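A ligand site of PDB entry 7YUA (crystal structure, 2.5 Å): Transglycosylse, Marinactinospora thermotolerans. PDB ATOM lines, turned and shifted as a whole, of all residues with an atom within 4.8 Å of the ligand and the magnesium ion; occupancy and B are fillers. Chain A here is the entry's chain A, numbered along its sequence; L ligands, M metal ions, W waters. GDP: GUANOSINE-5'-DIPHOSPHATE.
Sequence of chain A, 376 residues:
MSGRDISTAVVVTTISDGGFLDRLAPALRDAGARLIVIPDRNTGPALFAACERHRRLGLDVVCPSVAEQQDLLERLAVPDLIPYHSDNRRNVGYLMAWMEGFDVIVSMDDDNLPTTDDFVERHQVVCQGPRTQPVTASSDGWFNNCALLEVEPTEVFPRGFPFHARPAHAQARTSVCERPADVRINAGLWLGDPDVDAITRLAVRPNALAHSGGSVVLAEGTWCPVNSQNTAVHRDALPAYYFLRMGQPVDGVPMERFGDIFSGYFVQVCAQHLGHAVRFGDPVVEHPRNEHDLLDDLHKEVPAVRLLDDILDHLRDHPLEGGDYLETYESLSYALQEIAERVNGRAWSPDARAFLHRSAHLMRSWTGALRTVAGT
Residues that only touch the magnesium ion: Asp 109. Of the 22 residues printed, 3 come within 4 Å of the magnesium ion.
The magnesium ion is bound by an oxygen (O2B) of the ligand, at 2.1 Å. Slightly farther from the magnesium ion lies OD2 of Asp 111 (2.6 Å). Slightly farther from the magnesium ion lies a ring nitrogen (NE2) of His 287 (2.8 Å).
His 85 touches the ligand (C to O6, 3.3 Å). Asp 87 touches the ligand. Arg 89 touches the ligand. OD1 of Asp 109 touches C4' of the ligand, at 3.7 Å. CE1 of His 292 touches O1B of the ligand (3.3 Å). Hydrophobic or aromatic side chains within 4 Å of the ligand: Ile 15 and His 292. 16 residues have an atom within 4 Å of the ligand: Thr 13, Thr 14, Ile 15, Asp 40, Asn 42, His 85, Ser 86, Asp 87, Arg 89, Asp 109, Asp 110, Asp 111, Arg 257, His 287, Asn 290 and His 292. The nearest printed residue that does not touch the ligand is Arg 90 (4.03 Å).
Water W1 lies within hydrogen-bond range of N of Thr 13, NH1 of Arg 90 and O3' of the ligand.
The side-chain carboxylate (OD1) of Asp 40 lies within hydrogen-bond range of the backbone NH (N) of His 85, 2.8 Å away. OD2 of Asp 40 sits at hydrogen-bond distance from N of Ser 86 (3.0 Å). The side-chain carboxylate (OD1) of Asp 109 lies within salt-bridge range of the guanidinium group (NH1) of Arg 90, 3.2 Å away. A ring nitrogen (NE2) of His 292 sits close to the side-chain carboxylate (OD2) of Asp 297 (3.0 Å). The side-chain carboxylate (OD1) of Asp 297 lies within salt-bridge range of the guanidinium group (NH1) of Arg 257, at 3.5 Å. The backbone carbonyl oxygen (O) of Gln 229 sits at hydrogen-bond distance from the backbone NH (N) of Asp 109 (3.4 Å). The backbone NH (N) of Thr 14 lies within hydrogen-bond range of the backbone carbonyl oxygen (O) of Ile 38 (3.3 Å). The guanidinium group (NH2) of Arg 90 lies within salt-bridge range of the side-chain carboxylate (OD2) of Asp 87.
The side-chain carboxylate (OD2) of Asp 110 sits at hydrogen-bond distance from an oxygen (O2') of the ligand (2.6 Å). An oxygen (O6) of the ligand is in hydrogen-bond range of the side-chain amide nitrogen of Asn 42 (3.2 Å). The backbone carbonyl oxygen (O) of Thr 13 is in hydrogen-bond range of an oxygen (O3') of the ligand, 2.6 Å away. The side-chain hydroxyl (OG1) of Thr 14 lies close to an oxygen (O2') of the ligand (3.4 Å). An oxygen (O3B) of the ligand lies within salt-bridge range of the guanidinium group (NH2) of Arg 257 (3.5 Å). N2 of the ligand sits at hydrogen-bond distance from OG1 of Thr 13, 3.1 Å away. The backbone NH (N) of Asp 110 is in hydrogen-bond range of an oxygen (O3') of the ligand (3.2 Å). OD2 of Asp 40 is in hydrogen-bond range of N1 of the ligand (2.7 Å). The backbone NH (N) of Ile 15 lies within hydrogen-bond range of an oxygen (O2') of the ligand. A nitrogen (N2) of the ligand is in hydrogen-bond range of the backbone carbonyl oxygen (O) of Ser 86, 3.1 Å away. An oxygen (O1B) of the ligand sits close to the side-chain amide oxygen of Asn 290, at 3.3 Å.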
ATOM      1  N   VAL A  12      -9.373  25.238 -34.782  1.00  0.00           N
ATOM      2  CA  VAL A  12     -10.023  26.029 -33.744  1.00  0.00           C
ATOM      3  C   VAL A  12     -11.176  25.220 -33.178  1.00  0.00           C
ATOM      4  O   VAL A  12     -11.829  24.455 -33.909  1.00  0.00           O
ATOM      5  CB  VAL A  12     -10.535  27.374 -34.291  1.00  0.00           C
ATOM      6  CG1 VAL A  12     -11.357  28.075 -33.194  1.00  0.00           C
ATOM      7  CG2 VAL A  12      -9.394  28.227 -34.746  1.00  0.00           C
ATOM      8  N   THR A  13     -11.431  25.391 -31.895  1.00  0.00           N
ATOM      9  CA  THR A  13     -12.604  24.853 -31.245  1.00  0.00           C
ATOM     10  C   THR A  13     -13.336  26.005 -30.587  1.00  0.00           C
ATOM     11  O   THR A  13     -12.717  26.837 -29.922  1.00  0.00           O
ATOM     12  CB  THR A  13     -12.233  23.779 -30.220  1.00  0.00           C
ATOM     13  OG1 THR A  13     -13.382  22.983 -29.944  1.00  0.00           O
ATOM     14  CG2 THR A  13     -11.709  24.413 -28.929  1.00  0.00           C
ATOM     15  N   THR A  14     -14.647  26.078 -30.791  1.00  0.00           N
ATOM     16  CA  THR A  14     -15.368  27.256 -30.338  1.00  0.00           C
ATOM     17  C   THR A  14     -16.758  26.880 -29.862  1.00  0.00           C
ATOM     18  O   THR A  14     -17.363  25.926 -30.352  1.00  0.00           O
ATOM     19  CB  THR A  14     -15.475  28.310 -31.443  1.00  0.00           C
ATOM     20  OG1 THR A  14     -16.032  29.516 -30.904  1.00  0.00           O
ATOM     21  CG2 THR A  14     -16.384  27.808 -32.571  1.00  0.00           C
ATOM     22  N   ILE A  15     -17.252  27.662 -28.907  1.00  0.00           N
ATOM     23  CA  ILE A  15     -18.652  27.660 -28.528  1.00  0.00           C
ATOM     24  C   ILE A  15     -19.305  29.002 -28.856  1.00  0.00           C
ATOM     25  O   ILE A  15     -20.341  29.333 -28.298  1.00  0.00           O
ATOM     26  CB  ILE A  15     -18.844  27.312 -27.037  1.00  0.00           C
ATOM     27  CG1 ILE A  15     -18.006  28.262 -26.176  1.00  0.00           C
ATOM     28  CG2 ILE A  15     -18.492  25.872 -26.794  1.00  0.00           C
ATOM     29  CD1 ILE A  15     -17.998  27.926 -24.677  1.00  0.00           C
ATOM     30  N   ILE A  38     -14.003  23.124 -34.592  1.00  0.00           N
ATOM     31  CA  ILE A  38     -14.544  21.960 -33.896  1.00  0.00           C
ATOM     32  C   ILE A  38     -15.644  22.461 -32.947  1.00  0.00           C
ATOM     33  O   ILE A  38     -15.314  23.093 -31.924  1.00  0.00           O
ATOM     34  CB  ILE A  38     -13.469  21.186 -33.142  1.00  0.00           C
ATOM     35  CG1 ILE A  38     -12.426  20.642 -34.120  1.00  0.00           C
ATOM     36  CG2 ILE A  38     -14.106  20.061 -32.307  1.00  0.00           C
ATOM     37  CD1 ILE A  38     -12.950  19.558 -35.079  1.00  0.00           C
ATOM     38  N   PRO A  39     -16.906  22.223 -33.243  1.00  0.00           N
ATOM     39  CA  PRO A  39     -17.964  22.613 -32.316  1.00  0.00           C
ATOM     40  C   PRO A  39     -18.108  21.609 -31.188  1.00  0.00           C
ATOM     41  O   PRO A  39     -17.614  20.477 -31.257  1.00  0.00           O
ATOM     42  CB  PRO A  39     -19.209  22.640 -33.199  1.00  0.00           C
ATOM     43  CG  PRO A  39     -18.928  21.622 -34.250  1.00  0.00           C
ATOM     44  CD  PRO A  39     -17.438  21.613 -34.472  1.00  0.00           C
ATOM     45  N   ASP A  40     -18.786  22.053 -30.130  1.00  0.00           N
ATOM     46  CA  ASP A  40     -19.084  21.265 -28.950  1.00  0.00           C
ATOM     47  C   ASP A  40     -20.596  21.132 -28.781  1.00  0.00           C
ATOM     48  O   ASP A  40     -21.385  21.746 -29.514  1.00  0.00           O
ATOM     49  CB  ASP A  40     -18.472  21.898 -27.696  1.00  0.00           C
ATOM     50  CG  ASP A  40     -18.054  20.867 -26.665  1.00  0.00           C
ATOM     51  OD1 ASP A  40     -18.769  19.858 -26.480  1.00  0.00           O
ATOM     52  OD2 ASP A  40     -17.017  21.080 -26.021  1.00  0.00           O
ATOM     53  N   ASN A  42     -22.346  22.355 -26.501  1.00  0.00           N
ATOM     54  CA  ASN A  42     -22.829  23.677 -26.122  1.00  0.00           C
ATOM     55  C   ASN A  42     -22.547  24.749 -27.178  1.00  0.00           C
ATOM     56  O   ASN A  42     -22.475  25.938 -26.843  1.00  0.00           O
ATOM     57  CB  ASN A  42     -22.258  24.082 -24.753  1.00  0.00           C
ATOM     58  CG  ASN A  42     -20.725  23.881 -24.639  1.00  0.00           C
ATOM     59  OD1 ASN A  42     -20.128  23.055 -25.327  1.00  0.00           O
ATOM     60  ND2 ASN A  42     -20.105  24.644 -23.752  1.00  0.00           N
ATOM     61  N   HIS A  85     -18.108  19.686 -23.754  1.00  0.00           N
ATOM     62  CA  HIS A  85     -18.074  20.845 -22.854  1.00  0.00           C
ATOM     63  C   HIS A  85     -16.642  21.121 -22.403  1.00  0.00           C
ATOM     64  O   HIS A  85     -16.381  21.464 -21.237  1.00  0.00           O
ATOM     65  CB  HIS A  85     -18.992  20.628 -21.655  1.00  0.00           C
ATOM     66  CG  HIS A  85     -20.359  20.179 -22.026  1.00  0.00           C
ATOM     67  ND1 HIS A  85     -21.346  21.054 -22.423  1.00  0.00           N
ATOM     68  CD2 HIS A  85     -20.899  18.941 -22.110  1.00  0.00           C
ATOM     69  CE1 HIS A  85     -22.444  20.377 -22.709  1.00  0.00           C
ATOM     70  NE2 HIS A  85     -22.197  19.091 -22.532  1.00  0.00           N
ATOM     71  N   SER A  86     -15.701  20.943 -23.334  1.00  0.00           N
ATOM     72  CA  SER A  86     -14.289  21.197 -23.084  1.00  0.00           C
ATOM     73  C   SER A  86     -13.607  21.727 -24.337  1.00  0.00           C
ATOM     74  O   SER A  86     -13.943  21.319 -25.446  1.00  0.00           O
ATOM     75  CB  SER A  86     -13.558  19.947 -22.624  1.00  0.00           C
ATOM     76  OG  SER A  86     -12.272  20.296 -22.148  1.00  0.00           O
ATOM     77  N   ASP A  87     -12.637  22.628 -24.143  1.00  0.00           N
ATOM     78  CA  ASP A  87     -11.794  22.979 -25.279  1.00  0.00           C
ATOM     79  C   ASP A  87     -10.756  21.845 -25.604  1.00  0.00           C
ATOM     80  O   ASP A  87      -9.863  21.983 -26.496  1.00  0.00           O
ATOM     81  CB  ASP A  87     -11.088  24.321 -25.039  1.00  0.00           C
ATOM     82  CG  ASP A  87     -10.098  24.257 -23.897  1.00  0.00           C
ATOM     83  OD1 ASP A  87     -10.343  23.535 -22.908  1.00  0.00           O
ATOM     84  OD2 ASP A  87      -9.077  24.953 -23.982  1.00  0.00           O
ATOM     85  N   ARG A  89     -11.761  19.368 -27.134  1.00  0.00           N
ATOM     86  CA  ARG A  89     -12.194  18.966 -28.481  1.00  0.00           C
ATOM     87  C   ARG A  89     -11.260  19.489 -29.575  1.00  0.00           C
ATOM     88  O   ARG A  89     -11.338  19.025 -30.718  1.00  0.00           O
ATOM     89  CB  ARG A  89     -13.627  19.425 -28.743  1.00  0.00           C
ATOM     90  CG  ARG A  89     -14.626  18.911 -27.715  1.00  0.00           C
ATOM     91  CD  ARG A  89     -15.929  18.409 -28.330  1.00  0.00           C
ATOM     92  NE  ARG A  89     -15.737  17.270 -29.238  1.00  0.00           N
ATOM     93  CZ  ARG A  89     -15.633  15.997 -28.850  1.00  0.00           C
ATOM     94  NH1 ARG A  89     -15.705  15.656 -27.566  1.00  0.00           N
ATOM     95  NH2 ARG A  89     -15.463  15.042 -29.765  1.00  0.00           N
ATOM     96  N   ARG A  90     -10.410  20.452 -29.268  1.00  0.00           N
ATOM     97  CA  ARG A  90      -9.212  20.737 -30.058  1.00  0.00           C
ATOM     98  C   ARG A  90      -8.661  19.465 -30.710  1.00  0.00           C
ATOM     99  O   ARG A  90      -8.408  19.421 -31.912  1.00  0.00           O
ATOM    100  CB  ARG A  90      -8.143  21.291 -29.135  1.00  0.00           C
ATOM    101  CG  ARG A  90      -7.531  22.561 -29.485  1.00  0.00           C
ATOM    102  CD  ARG A  90      -6.727  22.997 -28.254  1.00  0.00           C
ATOM    103  NE  ARG A  90      -7.503  23.885 -27.389  1.00  0.00           N
ATOM    104  CZ  ARG A  90      -7.448  25.201 -27.458  1.00  0.00           C
ATOM    105  NH1 ARG A  90      -6.663  25.782 -28.365  1.00  0.00           N
ATOM    106  NH2 ARG A  90      -8.180  25.945 -26.616  1.00  0.00           N
ATOM    107  N   ASP A 109      -6.819  29.859 -30.867  1.00  0.00           N
ATOM    108  CA  ASP A 109      -8.088  30.170 -30.237  1.00  0.00           C
ATOM    109  C   ASP A 109      -8.965  30.963 -31.195  1.00  0.00           C
ATOM    110  O   ASP A 109      -8.479  31.581 -32.143  1.00  0.00           O
ATOM    111  CB  ASP A 109      -7.877  30.966 -28.946  1.00  0.00           C
ATOM    112  CG  ASP A 109      -7.353  30.114 -27.800  1.00  0.00           C
ATOM    113  OD1 ASP A 109      -7.462  28.861 -27.858  1.00  0.00           O
ATOM    114  OD2 ASP A 109      -6.853  30.714 -26.818  1.00  0.00           O
ATOM    115  N   ASP A 110     -10.264  30.934 -30.956  1.00  0.00           N
ATOM    116  CA  ASP A 110     -11.162  31.695 -31.807  1.00  0.00           C
ATOM    117  C   ASP A 110     -11.142  33.199 -31.520  1.00  0.00           C
ATOM    118  O   ASP A 110     -11.811  33.950 -32.233  1.00  0.00           O
ATOM    119  CB  ASP A 110     -12.597  31.154 -31.671  1.00  0.00           C
ATOM    120  CG  ASP A 110     -13.167  31.320 -30.281  1.00  0.00           C
ATOM    121  OD1 ASP A 110     -12.519  31.954 -29.424  1.00  0.00           O
ATOM    122  OD2 ASP A 110     -14.278  30.809 -30.034  1.00  0.00           O
ATOM    123  N   ASP A 111     -10.394  33.663 -30.523  1.00  0.00           N
ATOM    124  CA  ASP A 111     -10.280  35.100 -30.277  1.00  0.00           C
ATOM    125  C   ASP A 111      -8.950  35.704 -30.740  1.00  0.00           C
ATOM    126  O   ASP A 111      -8.825  36.918 -30.760  1.00  0.00           O
ATOM    127  CB  ASP A 111     -10.495  35.422 -28.780  1.00  0.00           C
ATOM    128  CG  ASP A 111      -9.605  34.592 -27.859  1.00  0.00           C
ATOM    129  OD1 ASP A 111      -8.845  33.740 -28.377  1.00  0.00           O
ATOM    130  OD2 ASP A 111      -9.675  34.803 -26.623  1.00  0.00           O
ATOM    131  N   GLN A 229      -2.331  28.590 -28.632  1.00  0.00           N
ATOM    132  CA  GLN A 229      -3.083  29.765 -29.078  1.00  0.00           C
ATOM    133  C   GLN A 229      -2.662  30.239 -30.474  1.00  0.00           C
ATOM    134  O   GLN A 229      -3.514  30.656 -31.266  1.00  0.00           O
ATOM    135  CB  GLN A 229      -2.916  30.912 -28.083  1.00  0.00           C
ATOM    136  CG  GLN A 229      -3.595  30.669 -26.733  1.00  0.00           C
ATOM    137  CD  GLN A 229      -3.558  31.900 -25.820  1.00  0.00           C
ATOM    138  OE1 GLN A 229      -2.931  32.931 -26.141  1.00  0.00           O
ATOM    139  NE2 GLN A 229      -4.227  31.803 -24.668  1.00  0.00           N
ATOM    140  N   ARG A 257      -7.092  24.702 -17.446  1.00  0.00           N
ATOM    141  CA  ARG A 257      -6.410  25.745 -18.185  1.00  0.00           C
ATOM    142  C   ARG A 257      -4.941  25.428 -18.487  1.00  0.00           C
ATOM    143  O   ARG A 257      -4.232  26.318 -19.011  1.00  0.00           O
ATOM    144  CB  ARG A 257      -6.507  27.084 -17.445  1.00  0.00           C
ATOM    145  CG  ARG A 257      -7.932  27.581 -17.210  1.00  0.00           C
ATOM    146  CD  ARG A 257      -7.980  28.907 -16.420  1.00  0.00           C
ATOM    147  NE  ARG A 257      -7.085  29.906 -16.997  1.00  0.00           N
ATOM    148  CZ  ARG A 257      -7.404  30.705 -18.008  1.00  0.00           C
ATOM    149  NH1 ARG A 257      -8.612  30.622 -18.561  1.00  0.00           N
ATOM    150  NH2 ARG A 257      -6.530  31.569 -18.474  1.00  0.00           N
ATOM    151  N   HIS A 287      -4.402  39.274 -29.231  1.00  0.00           N
ATOM    152  CA  HIS A 287      -5.221  38.635 -28.212  1.00  0.00           C
ATOM    153  C   HIS A 287      -5.932  39.720 -27.400  1.00  0.00           C
ATOM    154  O   HIS A 287      -5.265  40.446 -26.634  1.00  0.00           O
ATOM    155  CB  HIS A 287      -4.350  37.756 -27.305  1.00  0.00           C
ATOM    156  CG  HIS A 287      -5.108  36.876 -26.361  1.00  0.00           C
ATOM    157  ND1 HIS A 287      -4.495  36.153 -25.354  1.00  0.00           N
ATOM    158  CD2 HIS A 287      -6.439  36.596 -26.269  1.00  0.00           C
ATOM    159  CE1 HIS A 287      -5.404  35.473 -24.678  1.00  0.00           C
ATOM    160  NE2 HIS A 287      -6.593  35.726 -25.208  1.00  0.00           N
ATOM    161  N   ASN A 290      -9.745  39.747 -22.339  1.00  0.00           N
ATOM    162  CA  ASN A 290     -11.107  39.219 -22.048  1.00  0.00           C
ATOM    163  C   ASN A 290     -11.701  39.819 -20.762  1.00  0.00           C
ATOM    164  O   ASN A 290     -12.938  39.864 -20.687  1.00  0.00           O
ATOM    165  CB  ASN A 290     -11.099  37.689 -21.952  1.00  0.00           C
ATOM    166  CG  ASN A 290      -9.814  37.069 -22.461  1.00  0.00           C
ATOM    167  OD1 ASN A 290      -9.007  36.559 -21.686  1.00  0.00           O
ATOM    168  ND2 ASN A 290      -9.608  37.113 -23.771  1.00  0.00           N
ATOM    169  N   HIS A 292     -12.536  38.684 -17.579  1.00  0.00           N
ATOM    170  CA  HIS A 292     -13.688  37.967 -17.062  1.00  0.00           C
ATOM    171  C   HIS A 292     -13.514  37.755 -15.581  1.00  0.00           C
ATOM    172  O   HIS A 292     -13.778  38.686 -14.776  1.00  0.00           O
ATOM    173  CB  HIS A 292     -13.963  36.666 -17.848  1.00  0.00           C
ATOM    174  CG  HIS A 292     -12.827  35.668 -17.887  1.00  0.00           C
ATOM    175  ND1 HIS A 292     -11.549  35.968 -18.329  1.00  0.00           N
ATOM    176  CD2 HIS A 292     -12.823  34.341 -17.616  1.00  0.00           C
ATOM    177  CE1 HIS A 292     -10.804  34.876 -18.287  1.00  0.00           C
ATOM    178  NE2 HIS A 292     -11.558  33.877 -17.860  1.00  0.00           N
ATOM    179  N   ASP A 297      -9.910  32.000 -12.665  1.00  0.00           N
ATOM    180  CA  ASP A 297      -8.781  31.474 -13.431  1.00  0.00           C
ATOM    181  C   ASP A 297      -7.658  31.043 -12.510  1.00  0.00           C
ATOM    182  O   ASP A 297      -7.036  29.998 -12.722  1.00  0.00           O
ATOM    183  CB  ASP A 297      -8.254  32.508 -14.423  1.00  0.00           C
ATOM    184  CG  ASP A 297      -9.186  32.769 -15.553  1.00  0.00           C
ATOM    185  OD1 ASP A 297     -10.133  31.975 -15.713  1.00  0.00           O
ATOM    186  OD2 ASP A 297      -8.976  33.768 -16.270  1.00  0.00           O
HETATM  187  PB  GDP L   1      -8.855  32.678 -22.081  1.00  0.00           P
HETATM  188  O1B GDP L   1      -9.248  33.399 -20.827  1.00  0.00           O
HETATM  189  O2B GDP L   1      -8.794  33.527 -23.306  1.00  0.00           O
HETATM  190  O3B GDP L   1      -7.221  32.177 -21.837  1.00  0.00           O
HETATM  191  O3A GDP L   1      -9.779  31.247 -22.158  1.00  0.00           O
HETATM  192  PA  GDP L   1     -11.193  30.898 -22.904  1.00  0.00           P
HETATM  193  O1A GDP L   1     -11.809  32.050 -23.629  1.00  0.00           O
HETATM  194  O2A GDP L   1     -12.046  30.096 -21.986  1.00  0.00           O
HETATM  195  O5' GDP L   1     -11.050  29.705 -24.367  1.00  0.00           O
HETATM  196  C5' GDP L   1     -10.618  30.051 -25.622  1.00  0.00           C
HETATM  197  C4' GDP L   1     -10.969  28.914 -26.601  1.00  0.00           C
HETATM  198  O4' GDP L   1     -11.655  27.876 -25.963  1.00  0.00           O
HETATM  199  C3' GDP L   1     -11.923  29.511 -27.686  1.00  0.00           C
HETATM  200  O3' GDP L   1     -11.580  28.912 -28.918  1.00  0.00           O
HETATM  201  C2' GDP L   1     -13.309  29.050 -27.109  1.00  0.00           C
HETATM  202  O2' GDP L   1     -14.184  28.980 -28.136  1.00  0.00           O
HETATM  203  C1' GDP L   1     -12.903  27.634 -26.535  1.00  0.00           C
HETATM  204  N9  GDP L   1     -13.857  27.034 -25.556  1.00  0.00           N
HETATM  205  C8  GDP L   1     -14.184  27.599 -24.256  1.00  0.00           C
HETATM  206  N7  GDP L   1     -15.081  26.821 -23.607  1.00  0.00           N
HETATM  207  C5  GDP L   1     -15.325  25.716 -24.490  1.00  0.00           C
HETATM  208  C6  GDP L   1     -16.167  24.563 -24.336  1.00  0.00           C
HETATM  209  O6  GDP L   1     -16.901  24.289 -23.392  1.00  0.00           O
HETATM  210  N1  GDP L   1     -16.215  23.558 -25.452  1.00  0.00           N
HETATM  211  C2  GDP L   1     -15.420  23.762 -26.608  1.00  0.00           C
HETATM  212  N2  GDP L   1     -15.477  22.773 -27.667  1.00  0.00           N
HETATM  213  N3  GDP L   1     -14.625  24.841 -26.729  1.00  0.00           N
HETATM  214  C4  GDP L   1     -14.582  25.829 -25.669  1.00  0.00           C
HETATM  215 MG    MG M   1      -8.027  33.336 -25.209  1.00  0.00          MG
HETATM  216  O   HOH W   1      -9.423  26.555 -30.273  1.00  0.00           O
